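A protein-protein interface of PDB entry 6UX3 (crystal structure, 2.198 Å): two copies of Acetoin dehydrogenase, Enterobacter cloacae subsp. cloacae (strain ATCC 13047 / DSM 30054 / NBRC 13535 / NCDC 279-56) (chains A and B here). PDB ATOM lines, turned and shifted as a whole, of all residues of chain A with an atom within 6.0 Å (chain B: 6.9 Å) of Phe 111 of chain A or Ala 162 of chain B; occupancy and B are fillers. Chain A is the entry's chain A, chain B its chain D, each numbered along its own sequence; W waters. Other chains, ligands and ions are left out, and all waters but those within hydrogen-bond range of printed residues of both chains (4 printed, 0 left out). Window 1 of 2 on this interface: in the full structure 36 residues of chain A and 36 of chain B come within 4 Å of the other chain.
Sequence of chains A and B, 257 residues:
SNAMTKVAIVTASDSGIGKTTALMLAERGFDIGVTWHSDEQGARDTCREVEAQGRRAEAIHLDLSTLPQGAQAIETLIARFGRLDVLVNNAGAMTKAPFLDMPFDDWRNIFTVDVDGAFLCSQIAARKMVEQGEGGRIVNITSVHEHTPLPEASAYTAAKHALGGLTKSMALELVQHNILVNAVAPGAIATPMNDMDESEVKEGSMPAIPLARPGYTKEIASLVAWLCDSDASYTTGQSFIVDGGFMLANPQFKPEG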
ATOM      1  N   ASP A 106      -3.533  31.106   6.314  1.00  0.00           N
ATOM      2  CA  ASP A 106      -2.579  31.085   7.419  1.00  0.00           C
ATOM      3  C   ASP A 106      -3.119  30.273   8.590  1.00  0.00           C
ATOM      4  O   ASP A 106      -2.362  29.564   9.265  1.00  0.00           O
ATOM      5  CB  ASP A 106      -2.245  32.511   7.863  1.00  0.00           C
ATOM      6  CG  ASP A 106      -1.463  33.288   6.814  1.00  0.00           C
ATOM      7  OD1 ASP A 106      -1.169  32.724   5.737  1.00  0.00           O
ATOM      8  OD2 ASP A 106      -1.139  34.466   7.072  1.00  0.00           O
ATOM      9  N   TRP A 107      -4.426  30.363   8.846  1.00  0.00           N
ATOM     10  CA  TRP A 107      -5.034  29.546   9.891  1.00  0.00           C
ATOM     11  C   TRP A 107      -4.945  28.064   9.550  1.00  0.00           C
ATOM     12  O   TRP A 107      -4.627  27.239  10.414  1.00  0.00           O
ATOM     13  CB  TRP A 107      -6.486  29.981  10.094  1.00  0.00           C
ATOM     14  CG  TRP A 107      -7.390  28.979  10.757  1.00  0.00           C
ATOM     15  CD1 TRP A 107      -8.077  27.967  10.151  1.00  0.00           C
ATOM     16  CD2 TRP A 107      -7.744  28.927  12.143  1.00  0.00           C
ATOM     17  NE1 TRP A 107      -8.826  27.279  11.075  1.00  0.00           N
ATOM     18  CE2 TRP A 107      -8.637  27.848  12.307  1.00  0.00           C
ATOM     19  CE3 TRP A 107      -7.387  29.682  13.262  1.00  0.00           C
ATOM     20  CZ2 TRP A 107      -9.177  27.506  13.544  1.00  0.00           C
ATOM     21  CZ3 TRP A 107      -7.927  29.342  14.491  1.00  0.00           C
ATOM     22  CH2 TRP A 107      -8.810  28.265  14.621  1.00  0.00           C
ATOM     23  N   ARG A 108      -5.210  27.710   8.290  1.00  0.00           N
ATOM     24  CA  ARG A 108      -5.157  26.307   7.893  1.00  0.00           C
ATOM     25  C   ARG A 108      -3.729  25.779   7.828  1.00  0.00           C
ATOM     26  O   ARG A 108      -3.508  24.582   8.034  1.00  0.00           O
ATOM     27  CB  ARG A 108      -5.856  26.113   6.545  1.00  0.00           C
ATOM     28  CG  ARG A 108      -7.292  25.641   6.669  1.00  0.00           C
ATOM     29  CD  ARG A 108      -7.963  25.493   5.318  1.00  0.00           C
ATOM     30  NE  ARG A 108      -9.253  24.819   5.435  1.00  0.00           N
ATOM     31  CZ  ARG A 108     -10.103  24.637   4.429  1.00  0.00           C
ATOM     32  NH1 ARG A 108      -9.807  25.083   3.216  1.00  0.00           N
ATOM     33  NH2 ARG A 108     -11.252  24.009   4.636  1.00  0.00           N
ATOM     34  N   ASN A 109      -2.750  26.642   7.540  1.00  0.00           N
ATOM     35  CA  ASN A 109      -1.368  26.173   7.454  1.00  0.00           C
ATOM     36  C   ASN A 109      -0.818  25.812   8.829  1.00  0.00           C
ATOM     37  O   ASN A 109      -0.030  24.867   8.960  1.00  0.00           O
ATOM     38  CB  ASN A 109      -0.486  27.227   6.783  1.00  0.00           C
ATOM     39  CG  ASN A 109      -0.670  27.269   5.276  1.00  0.00           C
ATOM     40  OD1 ASN A 109      -1.079  26.282   4.659  1.00  0.00           O
ATOM     41  ND2 ASN A 109      -0.367  28.415   4.674  1.00  0.00           N
ATOM     42  N   ILE A 110      -1.221  26.549   9.866  1.00  0.00           N
ATOM     43  CA  ILE A 110      -0.761  26.229  11.212  1.00  0.00           C
ATOM     44  C   ILE A 110      -1.308  24.876  11.656  1.00  0.00           C
ATOM     45  O   ILE A 110      -0.586  24.070  12.252  1.00  0.00           O
ATOM     46  CB  ILE A 110      -1.132  27.364  12.186  1.00  0.00           C
ATOM     47  CG1 ILE A 110      -0.101  28.491  12.077  1.00  0.00           C
ATOM     48  CG2 ILE A 110      -1.209  26.857  13.616  1.00  0.00           C
ATOM     49  CD1 ILE A 110      -0.408  29.698  12.928  1.00  0.00           C
ATOM     50  N   PHE A 111      -2.575  24.585  11.340  1.00  0.00           N
ATOM     51  CA  PHE A 111      -3.105  23.255  11.624  1.00  0.00           C
ATOM     52  C   PHE A 111      -2.386  22.181  10.815  1.00  0.00           C
ATOM     53  O   PHE A 111      -2.192  21.063  11.305  1.00  0.00           O
ATOM     54  CB  PHE A 111      -4.612  23.211  11.355  1.00  0.00           C
ATOM     55  CG  PHE A 111      -5.451  23.630  12.537  1.00  0.00           C
ATOM     56  CD1 PHE A 111      -5.731  24.969  12.771  1.00  0.00           C
ATOM     57  CD2 PHE A 111      -5.952  22.685  13.417  1.00  0.00           C
ATOM     58  CE1 PHE A 111      -6.492  25.355  13.858  1.00  0.00           C
ATOM     59  CE2 PHE A 111      -6.718  23.068  14.510  1.00  0.00           C
ATOM     60  CZ  PHE A 111      -6.988  24.402  14.729  1.00  0.00           C
ATOM     61  N   THR A 112      -1.968  22.499   9.585  1.00  0.00           N
ATOM     62  CA  THR A 112      -1.243  21.518   8.782  1.00  0.00           C
ATOM     63  C   THR A 112       0.094  21.158   9.424  1.00  0.00           C
ATOM     64  O   THR A 112       0.461  19.980   9.496  1.00  0.00           O
ATOM     65  CB  THR A 112      -1.036  22.045   7.362  1.00  0.00           C
ATOM     66  OG1 THR A 112      -2.309  22.237   6.733  1.00  0.00           O
ATOM     67  CG2 THR A 112      -0.215  21.060   6.535  1.00  0.00           C
ATOM     68  N   VAL A 113       0.814  22.157   9.928  1.00  0.00           N
ATOM     69  CA  VAL A 113       2.125  21.905  10.513  1.00  0.00           C
ATOM     70  C   VAL A 113       2.021  21.381  11.946  1.00  0.00           C
ATOM     71  O   VAL A 113       2.831  20.540  12.359  1.00  0.00           O
ATOM     72  CB  VAL A 113       2.967  23.190  10.434  1.00  0.00           C
ATOM     73  CG1 VAL A 113       4.179  23.109  11.350  1.00  0.00           C
ATOM     74  CG2 VAL A 113       3.400  23.431   9.001  1.00  0.00           C
ATOM     75  N   ASP A 114       1.030  21.835  12.716  1.00  0.00           N
ATOM     76  CA  ASP A 114       1.002  21.604  14.156  1.00  0.00           C
ATOM     77  C   ASP A 114       0.085  20.465  14.595  1.00  0.00           C
ATOM     78  O   ASP A 114       0.096  20.116  15.780  1.00  0.00           O
ATOM     79  CB  ASP A 114       0.598  22.887  14.895  1.00  0.00           C
ATOM     80  CG  ASP A 114       1.712  23.920  14.915  1.00  0.00           C
ATOM     81  OD1 ASP A 114       2.802  23.626  14.387  1.00  0.00           O
ATOM     82  OD2 ASP A 114       1.498  25.025  15.461  1.00  0.00           O
ATOM     83  N   VAL A 115      -0.708  19.877  13.699  1.00  0.00           N
ATOM     84  CA  VAL A 115      -1.497  18.716  14.103  1.00  0.00           C
ATOM     85  C   VAL A 115      -1.669  17.731  12.947  1.00  0.00           C
ATOM     86  O   VAL A 115      -1.702  16.516  13.166  1.00  0.00           O
ATOM     87  CB  VAL A 115      -2.856  19.145  14.701  1.00  0.00           C
ATOM     88  CG1 VAL A 115      -3.776  19.734  13.654  1.00  0.00           C
ATOM     89  CG2 VAL A 115      -3.526  17.972  15.414  1.00  0.00           C
ATOM     90  N   ASP A 116      -1.759  18.233  11.709  1.00  0.00           N
ATOM     91  CA  ASP A 116      -1.966  17.336  10.570  1.00  0.00           C
ATOM     92  C   ASP A 116      -0.765  16.426  10.350  1.00  0.00           C
ATOM     93  O   ASP A 116      -0.925  15.220  10.124  1.00  0.00           O
ATOM     94  CB  ASP A 116      -2.259  18.139   9.303  1.00  0.00           C
ATOM     95  CG  ASP A 116      -3.662  18.711   9.285  1.00  0.00           C
ATOM     96  OD1 ASP A 116      -4.449  18.389  10.202  1.00  0.00           O
ATOM     97  OD2 ASP A 116      -3.975  19.484   8.353  1.00  0.00           O
ATOM     98  N   GLY A 117       0.446  16.987  10.411  1.00  0.00           N
ATOM     99  CA  GLY A 117       1.639  16.170  10.256  1.00  0.00           C
ATOM    100  C   GLY A 117       1.755  15.089  11.312  1.00  0.00           C
ATOM    101  O   GLY A 117       2.025  13.927  10.998  1.00  0.00           O
ATOM    102  N   SER A 154      -3.984  32.687  18.087  1.00  0.00           N
ATOM    103  CA  SER A 154      -5.184  31.871  18.253  1.00  0.00           C
ATOM    104  C   SER A 154      -5.086  30.563  17.474  1.00  0.00           C
ATOM    105  O   SER A 154      -5.546  29.516  17.947  1.00  0.00           O
ATOM    106  CB  SER A 154      -6.415  32.671  17.820  1.00  0.00           C
ATOM    107  OG  SER A 154      -6.278  33.129  16.486  1.00  0.00           O
ATOM    108  N   ALA A 155      -4.495  30.598  16.276  1.00  0.00           N
ATOM    109  CA  ALA A 155      -4.371  29.373  15.493  1.00  0.00           C
ATOM    110  C   ALA A 155      -3.377  28.406  16.128  1.00  0.00           C
ATOM    111  O   ALA A 155      -3.599  27.190  16.122  1.00  0.00           O
ATOM    112  CB  ALA A 155      -3.954  29.700  14.060  1.00  0.00           C
ATOM    113  N   THR A 157      -2.713  28.226  19.340  1.00  0.00           N
ATOM    114  CA  THR A 157      -3.377  27.712  20.531  1.00  0.00           C
ATOM    115  C   THR A 157      -4.409  26.651  20.172  1.00  0.00           C
ATOM    116  O   THR A 157      -4.513  25.623  20.850  1.00  0.00           O
ATOM    117  CB  THR A 157      -4.029  28.868  21.287  1.00  0.00           C
ATOM    118  OG1 THR A 157      -3.019  29.801  21.693  1.00  0.00           O
ATOM    119  CG2 THR A 157      -4.779  28.366  22.516  1.00  0.00           C
ATOM    120  N   ALA A 158      -5.170  26.876  19.099  1.00  0.00           N
ATOM    121  CA  ALA A 158      -6.196  25.915  18.714  1.00  0.00           C
ATOM    122  C   ALA A 158      -5.579  24.622  18.191  1.00  0.00           C
ATOM    123  O   ALA A 158      -6.081  23.530  18.480  1.00  0.00           O
ATOM    124  CB  ALA A 158      -7.128  26.537  17.672  1.00  0.00           C
ATOM    125  N   ALA A 159      -4.492  24.723  17.421  1.00  0.00           N
ATOM    126  CA  ALA A 159      -3.831  23.522  16.914  1.00  0.00           C
ATOM    127  C   ALA A 159      -3.205  22.713  18.045  1.00  0.00           C
ATOM    128  O   ALA A 159      -3.241  21.476  18.027  1.00  0.00           O
ATOM    129  CB  ALA A 159      -2.776  23.898  15.875  1.00  0.00           C
ATOM    130  N   HIS A 161      -4.345  22.620  21.111  1.00  0.00           N
ATOM    131  CA  HIS A 161      -5.476  21.948  21.753  1.00  0.00           C
ATOM    132  C   HIS A 161      -5.927  20.735  20.946  1.00  0.00           C
ATOM    133  O   HIS A 161      -6.291  19.698  21.517  1.00  0.00           O
ATOM    134  CB  HIS A 161      -6.647  22.916  21.925  1.00  0.00           C
ATOM    135  CG  HIS A 161      -6.528  23.832  23.103  1.00  0.00           C
ATOM    136  ND1 HIS A 161      -5.493  24.728  23.248  1.00  0.00           N
ATOM    137  CD2 HIS A 161      -7.341  24.019  24.170  1.00  0.00           C
ATOM    138  CE1 HIS A 161      -5.664  25.416  24.363  1.00  0.00           C
ATOM    139  NE2 HIS A 161      -6.779  25.006  24.940  1.00  0.00           N
ATOM    140  N   ALA A 162      -5.928  20.851  19.615  1.00  0.00           N
ATOM    141  CA  ALA A 162      -6.314  19.729  18.766  1.00  0.00           C
ATOM    142  C   ALA A 162      -5.350  18.561  18.919  1.00  0.00           C
ATOM    143  O   ALA A 162      -5.772  17.400  18.972  1.00  0.00           O
ATOM    144  CB  ALA A 162      -6.375  20.170  17.303  1.00  0.00           C
ATOM    145  N   TRP B 107     -10.370  13.450   7.682  1.00  0.00           N
ATOM    146  CA  TRP B 107      -9.826  14.143   8.843  1.00  0.00           C
ATOM    147  C   TRP B 107      -9.895  15.653   8.653  1.00  0.00           C
ATOM    148  O   TRP B 107     -10.360  16.382   9.536  1.00  0.00           O
ATOM    149  CB  TRP B 107      -8.388  13.674   9.084  1.00  0.00           C
ATOM    150  CG  TRP B 107      -7.550  14.590   9.928  1.00  0.00           C
ATOM    151  CD1 TRP B 107      -6.810  15.654   9.496  1.00  0.00           C
ATOM    152  CD2 TRP B 107      -7.344  14.510  11.344  1.00  0.00           C
ATOM    153  NE1 TRP B 107      -6.167  16.247  10.555  1.00  0.00           N
ATOM    154  CE2 TRP B 107      -6.477  15.563  11.701  1.00  0.00           C
ATOM    155  CE3 TRP B 107      -7.812  13.653  12.344  1.00  0.00           C
ATOM    156  CZ2 TRP B 107      -6.068  15.784  13.019  1.00  0.00           C
ATOM    157  CZ3 TRP B 107      -7.406  13.873  13.653  1.00  0.00           C
ATOM    158  CH2 TRP B 107      -6.544  14.932  13.977  1.00  0.00           C
ATOM    159  N   ARG B 108      -9.456  16.141   7.491  1.00  0.00           N
ATOM    160  CA  ARG B 108      -9.507  17.575   7.244  1.00  0.00           C
ATOM    161  C   ARG B 108     -10.937  18.075   7.083  1.00  0.00           C
ATOM    162  O   ARG B 108     -11.232  19.218   7.453  1.00  0.00           O
ATOM    163  CB  ARG B 108      -8.672  17.932   6.015  1.00  0.00           C
ATOM    164  CG  ARG B 108      -7.176  17.884   6.265  1.00  0.00           C
ATOM    165  CD  ARG B 108      -6.400  18.483   5.110  1.00  0.00           C
ATOM    166  NE  ARG B 108      -5.111  19.011   5.548  1.00  0.00           N
ATOM    167  CZ  ARG B 108      -4.199  19.534   4.734  1.00  0.00           C
ATOM    168  NH1 ARG B 108      -4.425  19.599   3.427  1.00  0.00           N
ATOM    169  NH2 ARG B 108      -3.055  19.990   5.228  1.00  0.00           N
ATOM    170  N   PHE B 111     -12.419  18.861  10.477  1.00  0.00           N
ATOM    171  CA  PHE B 111     -11.934  20.138  10.984  1.00  0.00           C
ATOM    172  C   PHE B 111     -12.598  21.314  10.277  1.00  0.00           C
ATOM    173  O   PHE B 111     -12.810  22.364  10.894  1.00  0.00           O
ATOM    174  CB  PHE B 111     -10.414  20.211  10.847  1.00  0.00           C
ATOM    175  CG  PHE B 111      -9.673  19.617  12.010  1.00  0.00           C
ATOM    176  CD1 PHE B 111      -9.590  18.244  12.172  1.00  0.00           C
ATOM    177  CD2 PHE B 111      -9.059  20.437  12.945  1.00  0.00           C
ATOM    178  CE1 PHE B 111      -8.904  17.697  13.249  1.00  0.00           C
ATOM    179  CE2 PHE B 111      -8.377  19.899  14.018  1.00  0.00           C
ATOM    180  CZ  PHE B 111      -8.298  18.526  14.170  1.00  0.00           C
ATOM    181  N   ASP B 114     -16.212  21.563  11.862  1.00  0.00           N
ATOM    182  CA  ASP B 114     -16.284  21.636  13.314  1.00  0.00           C
ATOM    183  C   ASP B 114     -15.422  22.731  13.931  1.00  0.00           C
ATOM    184  O   ASP B 114     -15.572  22.999  15.128  1.00  0.00           O
ATOM    185  CB  ASP B 114     -15.903  20.286  13.933  1.00  0.00           C
ATOM    186  CG  ASP B 114     -17.041  19.276  13.881  1.00  0.00           C
ATOM    187  OD1 ASP B 114     -18.200  19.664  14.141  1.00  0.00           O
ATOM    188  OD2 ASP B 114     -16.774  18.091  13.582  1.00  0.00           O
ATOM    189  N   VAL B 115     -14.532  23.375  13.174  1.00  0.00           N
ATOM    190  CA  VAL B 115     -13.798  24.493  13.764  1.00  0.00           C
ATOM    191  C   VAL B 115     -13.488  25.575  12.730  1.00  0.00           C
ATOM    192  O   VAL B 115     -13.484  26.768  13.058  1.00  0.00           O
ATOM    193  CB  VAL B 115     -12.521  24.005  14.487  1.00  0.00           C
ATOM    194  CG1 VAL B 115     -11.460  23.529  13.518  1.00  0.00           C
ATOM    195  CG2 VAL B 115     -11.977  25.103  15.385  1.00  0.00           C
ATOM    196  N   ASP B 116     -13.250  25.187  11.472  1.00  0.00           N
ATOM    197  CA  ASP B 116     -12.975  26.190  10.444  1.00  0.00           C
ATOM    198  C   ASP B 116     -14.182  27.091  10.211  1.00  0.00           C
ATOM    199  O   ASP B 116     -14.033  28.311  10.058  1.00  0.00           O
ATOM    200  CB  ASP B 116     -12.550  25.520   9.136  1.00  0.00           C
ATOM    201  CG  ASP B 116     -11.165  24.891   9.214  1.00  0.00           C
ATOM    202  OD1 ASP B 116     -10.369  25.280  10.099  1.00  0.00           O
ATOM    203  OD2 ASP B 116     -10.868  24.012   8.376  1.00  0.00           O
ATOM    204  N   GLU B 146     -14.733  18.047  23.945  1.00  0.00           N
ATOM    205  CA  GLU B 146     -13.695  19.060  24.043  1.00  0.00           C
ATOM    206  C   GLU B 146     -12.703  18.721  25.152  1.00  0.00           C
ATOM    207  O   GLU B 146     -11.572  19.217  25.135  1.00  0.00           O
ATOM    208  CB  GLU B 146     -14.339  20.434  24.279  1.00  0.00           C
ATOM    209  CG  GLU B 146     -13.359  21.576  24.491  1.00  0.00           C
ATOM    210  CD  GLU B 146     -13.998  22.783  25.150  1.00  0.00           C
ATOM    211  OE1 GLU B 146     -15.243  22.914  25.107  1.00  0.00           O
ATOM    212  OE2 GLU B 146     -13.248  23.604  25.716  1.00  0.00           O
ATOM    213  N   TYR B 156     -13.200  14.086  15.392  1.00  0.00           N
ATOM    214  CA  TYR B 156     -14.226  14.867  16.073  1.00  0.00           C
ATOM    215  C   TYR B 156     -13.720  15.362  17.422  1.00  0.00           C
ATOM    216  O   TYR B 156     -13.923  16.527  17.783  1.00  0.00           O
ATOM    217  CB  TYR B 156     -15.486  14.012  16.239  1.00  0.00           C
ATOM    218  CG  TYR B 156     -16.591  14.633  17.070  1.00  0.00           C
ATOM    219  CD1 TYR B 156     -17.551  15.448  16.484  1.00  0.00           C
ATOM    220  CD2 TYR B 156     -16.694  14.373  18.432  1.00  0.00           C
ATOM    221  CE1 TYR B 156     -18.570  16.009  17.235  1.00  0.00           C
ATOM    222  CE2 TYR B 156     -17.713  14.930  19.191  1.00  0.00           C
ATOM    223  CZ  TYR B 156     -18.647  15.749  18.585  1.00  0.00           C
ATOM    224  OH  TYR B 156     -19.666  16.310  19.323  1.00  0.00           O
ATOM    225  N   THR B 157     -13.045  14.489  18.172  1.00  0.00           N
ATOM    226  CA  THR B 157     -12.471  14.884  19.453  1.00  0.00           C
ATOM    227  C   THR B 157     -11.423  15.973  19.273  1.00  0.00           C
ATOM    228  O   THR B 157     -11.468  17.011  19.945  1.00  0.00           O
ATOM    229  CB  THR B 157     -11.865  13.661  20.140  1.00  0.00           C
ATOM    230  OG1 THR B 157     -12.891  12.682  20.357  1.00  0.00           O
ATOM    231  CG2 THR B 157     -11.233  14.047  21.475  1.00  0.00           C
ATOM    232  N   ALA B 158     -10.470  15.757  18.361  1.00  0.00           N
ATOM    233  CA  ALA B 158      -9.422  16.748  18.138  1.00  0.00           C
ATOM    234  C   ALA B 158     -10.008  18.089  17.715  1.00  0.00           C
ATOM    235  O   ALA B 158      -9.523  19.145  18.136  1.00  0.00           O
ATOM    236  CB  ALA B 158      -8.433  16.244  17.089  1.00  0.00           C
ATOM    237  N   ALA B 159     -11.059  18.070  16.891  1.00  0.00           N
ATOM    238  CA  ALA B 159     -11.627  19.326  16.415  1.00  0.00           C
ATOM    239  C   ALA B 159     -12.390  20.044  17.523  1.00  0.00           C
ATOM    240  O   ALA B 159     -12.361  21.279  17.598  1.00  0.00           O
ATOM    241  CB  ALA B 159     -12.528  19.073  15.208  1.00  0.00           C
ATOM    242  N   LYS B 160     -13.080  19.291  18.387  1.00  0.00           N
ATOM    243  CA  LYS B 160     -13.747  19.900  19.537  1.00  0.00           C
ATOM    244  C   LYS B 160     -12.743  20.530  20.494  1.00  0.00           C
ATOM    245  O   LYS B 160     -12.994  21.612  21.040  1.00  0.00           O
ATOM    246  CB  LYS B 160     -14.592  18.863  20.272  1.00  0.00           C
ATOM    247  CG  LYS B 160     -15.846  18.467  19.536  1.00  0.00           C
ATOM    248  CD  LYS B 160     -16.691  19.685  19.242  1.00  0.00           C
ATOM    249  CE  LYS B 160     -17.860  19.318  18.351  1.00  0.00           C
ATOM    250  NZ  LYS B 160     -18.686  20.505  18.042  1.00  0.00           N
ATOM    251  N   HIS B 161     -11.611  19.858  20.732  1.00  0.00           N
ATOM    252  CA  HIS B 161     -10.545  20.477  21.514  1.00  0.00           C
ATOM    253  C   HIS B 161     -10.073  21.766  20.856  1.00  0.00           C
ATOM    254  O   HIS B 161      -9.884  22.786  21.532  1.00  0.00           O
ATOM    255  CB  HIS B 161      -9.370  19.513  21.676  1.00  0.00           C
ATOM    256  CG  HIS B 161      -9.543  18.500  22.767  1.00  0.00           C
ATOM    257  ND1 HIS B 161     -10.553  17.560  22.761  1.00  0.00           N
ATOM    258  CD2 HIS B 161      -8.809  18.254  23.881  1.00  0.00           C
ATOM    259  CE1 HIS B 161     -10.441  16.790  23.830  1.00  0.00           C
ATOM    260  NE2 HIS B 161      -9.391  17.192  24.525  1.00  0.00           N
ATOM    261  N   ALA B 162      -9.877  21.733  19.533  1.00  0.00           N
ATOM    262  CA  ALA B 162      -9.432  22.912  18.795  1.00  0.00           C
ATOM    263  C   ALA B 162     -10.393  24.077  18.975  1.00  0.00           C
ATOM    264  O   ALA B 162      -9.966  25.215  19.203  1.00  0.00           O
ATOM    265  CB  ALA B 162      -9.287  22.572  17.312  1.00  0.00           C
ATOM    266  N   LEU B 163     -11.698  23.816  18.858  1.00  0.00           N
ATOM    267  CA  LEU B 163     -12.685  24.867  19.071  1.00  0.00           C
ATOM    268  C   LEU B 163     -12.683  25.343  20.520  1.00  0.00           C
ATOM    269  O   LEU B 163     -12.920  26.529  20.783  1.00  0.00           O
ATOM    270  CB  LEU B 163     -14.070  24.363  18.658  1.00  0.00           C
ATOM    271  CG  LEU B 163     -15.212  25.377  18.692  1.00  0.00           C
ATOM    272  CD1 LEU B 163     -14.791  26.675  18.010  1.00  0.00           C
ATOM    273  CD2 LEU B 163     -16.466  24.807  18.038  1.00  0.00           C
ATOM    274  N   GLY B 164     -12.399  24.445  21.465  1.00  0.00           N
ATOM    275  CA  GLY B 164     -12.185  24.873  22.839  1.00  0.00           C
ATOM    276  C   GLY B 164     -11.007  25.820  22.980  1.00  0.00           C
ATOM    277  O   GLY B 164     -11.066  26.788  23.744  1.00  0.00           O
ATOM    278  N   GLY B 165      -9.920  25.554  22.252  1.00  0.00           N
ATOM    279  CA  GLY B 165      -8.779  26.455  22.298  1.00  0.00           C
ATOM    280  C   GLY B 165      -9.063  27.791  21.639  1.00  0.00           C
ATOM    281  O   GLY B 165      -8.666  28.843  22.148  1.00  0.00           O
ATOM    282  N   LEU B 166      -9.756  27.767  20.498  1.00  0.00           N
ATOM    283  CA  LEU B 166     -10.147  29.012  19.846  1.00  0.00           C
ATOM    284  C   LEU B 166     -11.041  29.856  20.744  1.00  0.00           C
ATOM    285  O   LEU B 166     -10.928  31.088  20.747  1.00  0.00           O
ATOM    286  CB  LEU B 166     -10.845  28.708  18.522  1.00  0.00           C
ATOM    287  CG  LEU B 166     -11.360  29.895  17.703  1.00  0.00           C
ATOM    288  CD1 LEU B 166     -10.244  30.879  17.377  1.00  0.00           C
ATOM    289  CD2 LEU B 166     -12.024  29.399  16.433  1.00  0.00           C
ATOM    290  N   THR B 167     -11.919  29.218  21.524  1.00  0.00           N
ATOM    291  CA  THR B 167     -12.786  29.966  22.433  1.00  0.00           C
ATOM    292  C   THR B 167     -11.968  30.755  23.446  1.00  0.00           C
ATOM    293  O   THR B 167     -12.264  31.925  23.713  1.00  0.00           O
ATOM    294  CB  THR B 167     -13.750  29.023  23.155  1.00  0.00           C
ATOM    295  OG1 THR B 167     -14.560  28.336  22.199  1.00  0.00           O
ATOM    296  CG2 THR B 167     -14.644  29.790  24.111  1.00  0.00           C
HETATM  297  O   HOH W   1      -7.020  19.406  10.222  1.00  0.00           O
HETATM  298  O   HOH W   2      -5.365  22.498   5.125  1.00  0.00           O
HETATM  299  O   HOH W   3      -8.340  23.961  10.659  1.00  0.00           O
HETATM  300  O   HOH W   4      -4.887  21.804   7.477  1.00  0.00           O
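Arg 108 of chain A touches Asp 116 of chain B, and with the chains exchanged Asp 116 of chain A touches Arg 108 of chain B.
Phe 111 of chain B touches its own counterpart, Phe 111 of chain A.
His 161 of chain A touches its own counterpart, His 161 of chain B.
Ala 162 of chain B touches its own counterpart, Ala 162 of chain A.
11 positions are printed for both chains.
Water W3 bridges OD1 of Asp 116 of chain B (2.5 Å) and NE1 of Trp 107 of chain A (3.4 Å).
Water W1 lies within hydrogen-bond range of the side-chain carboxylate (OD1) of Asp 116 of chain A (2.8 Å) and the indole nitrogen (NE1) of Trp 107 of chain B (3.3 Å).
The indole nitrogen (NE1) of Trp 107 of chain A is in hydrogen-bond range of the side-chain carboxylate (OD1) of Asp 116 of chain B (2.7 Å).
NE of Arg 108 of chain A is in salt-bridge range of OD2 of Asp 116 of chain B (3.5 Å).
The side-chain hydroxyl (OG1) of Thr 112 of chain A sits at hydrogen-bond distance from the guanidinium group (NH2) of Arg 108 of chain B (2.8 Å).
The side-chain carboxylate of Asp 116 of chain A is in hydrogen-bond range of the indole nitrogen of Trp 107 of chain B (2.8 Å).
The side-chain carboxylate (OD2) of Asp 116 of chain A is in salt-bridge range of the guanidinium group (NE) of Arg 108 of chain B (3.1 Å).
Hydrophobic or aromatic side chains of chain A within 4 Å of the printed part of chain B: Trp 107, Phe 111, Ala 158, His 161 and Ala 162.
Among the printed residues, 15 pairs touch across the chains.
Among the printed residues, Asp or Glu carboxylates within 4 Å of a Lys or Arg side-chain nitrogen of the other chain: Arg 108 of chain A with Asp 116 of chain B (3.5 Å) and Asp 116 of chain A with Arg 108 of chain B (3.1 Å).
Of chain B, only Phe 111 (3.6 Å) and Ala 162 (3.8 Å) come within 4 Å of Phe 111 of chain A.
Of chain A, only Phe 111, Ala 158 and Ala 162 come within 4 Å of Ala 162 of chain B.
Of the printed residues of chain A, Asp 116 of chain B touches Trp 107 (2.7 Å) and Arg 108 (3.5 Å).
Of the printed residues of chain B, Asp 116 of chain A touches Trp 107 (2.8 Å) and Arg 108 (3.1 Å).
Of the printed residues of chain B, Thr 157 of chain A touches Gly 165 (3.9 Å).
Leu 163 of chain B touches none of the printed residues of chain A.
The nearest printed residue of chain B that does not touch Trp 107 of chain A is Val 115 of chain B (4.1 Å).
Leu 166 of chain B touches Trp 107 of chain A (CD2 to CH2, 3.9 Å).
CE2 of Phe 111 of chain A touches CE2 of Phe 111 of chain B, 3.6 Å away.
O of Gly 165 of chain B touches CG2 of Thr 157 of chain A, 3.9 Å away.
CA of Gly 165 of chain B touches CD2 of His 161 of chain A, at 3.4 Å.
Ala 162 of chain A touches Ala 158 of chain B.
O of Phe 111 of chain A sits at hydrogen-bond distance from N of Asp 116 of chain A, at 2.9 Å.
A ring nitrogen (ND1) of His 161 of chain A lies within hydrogen-bond range of the backbone carbonyl oxygen (O) of Thr 157 of chain A, 2.7 Å away.
O of Thr 157 of chain B is in hydrogen-bond range of ND1 of His 161 of chain B, at 3.0 Å.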
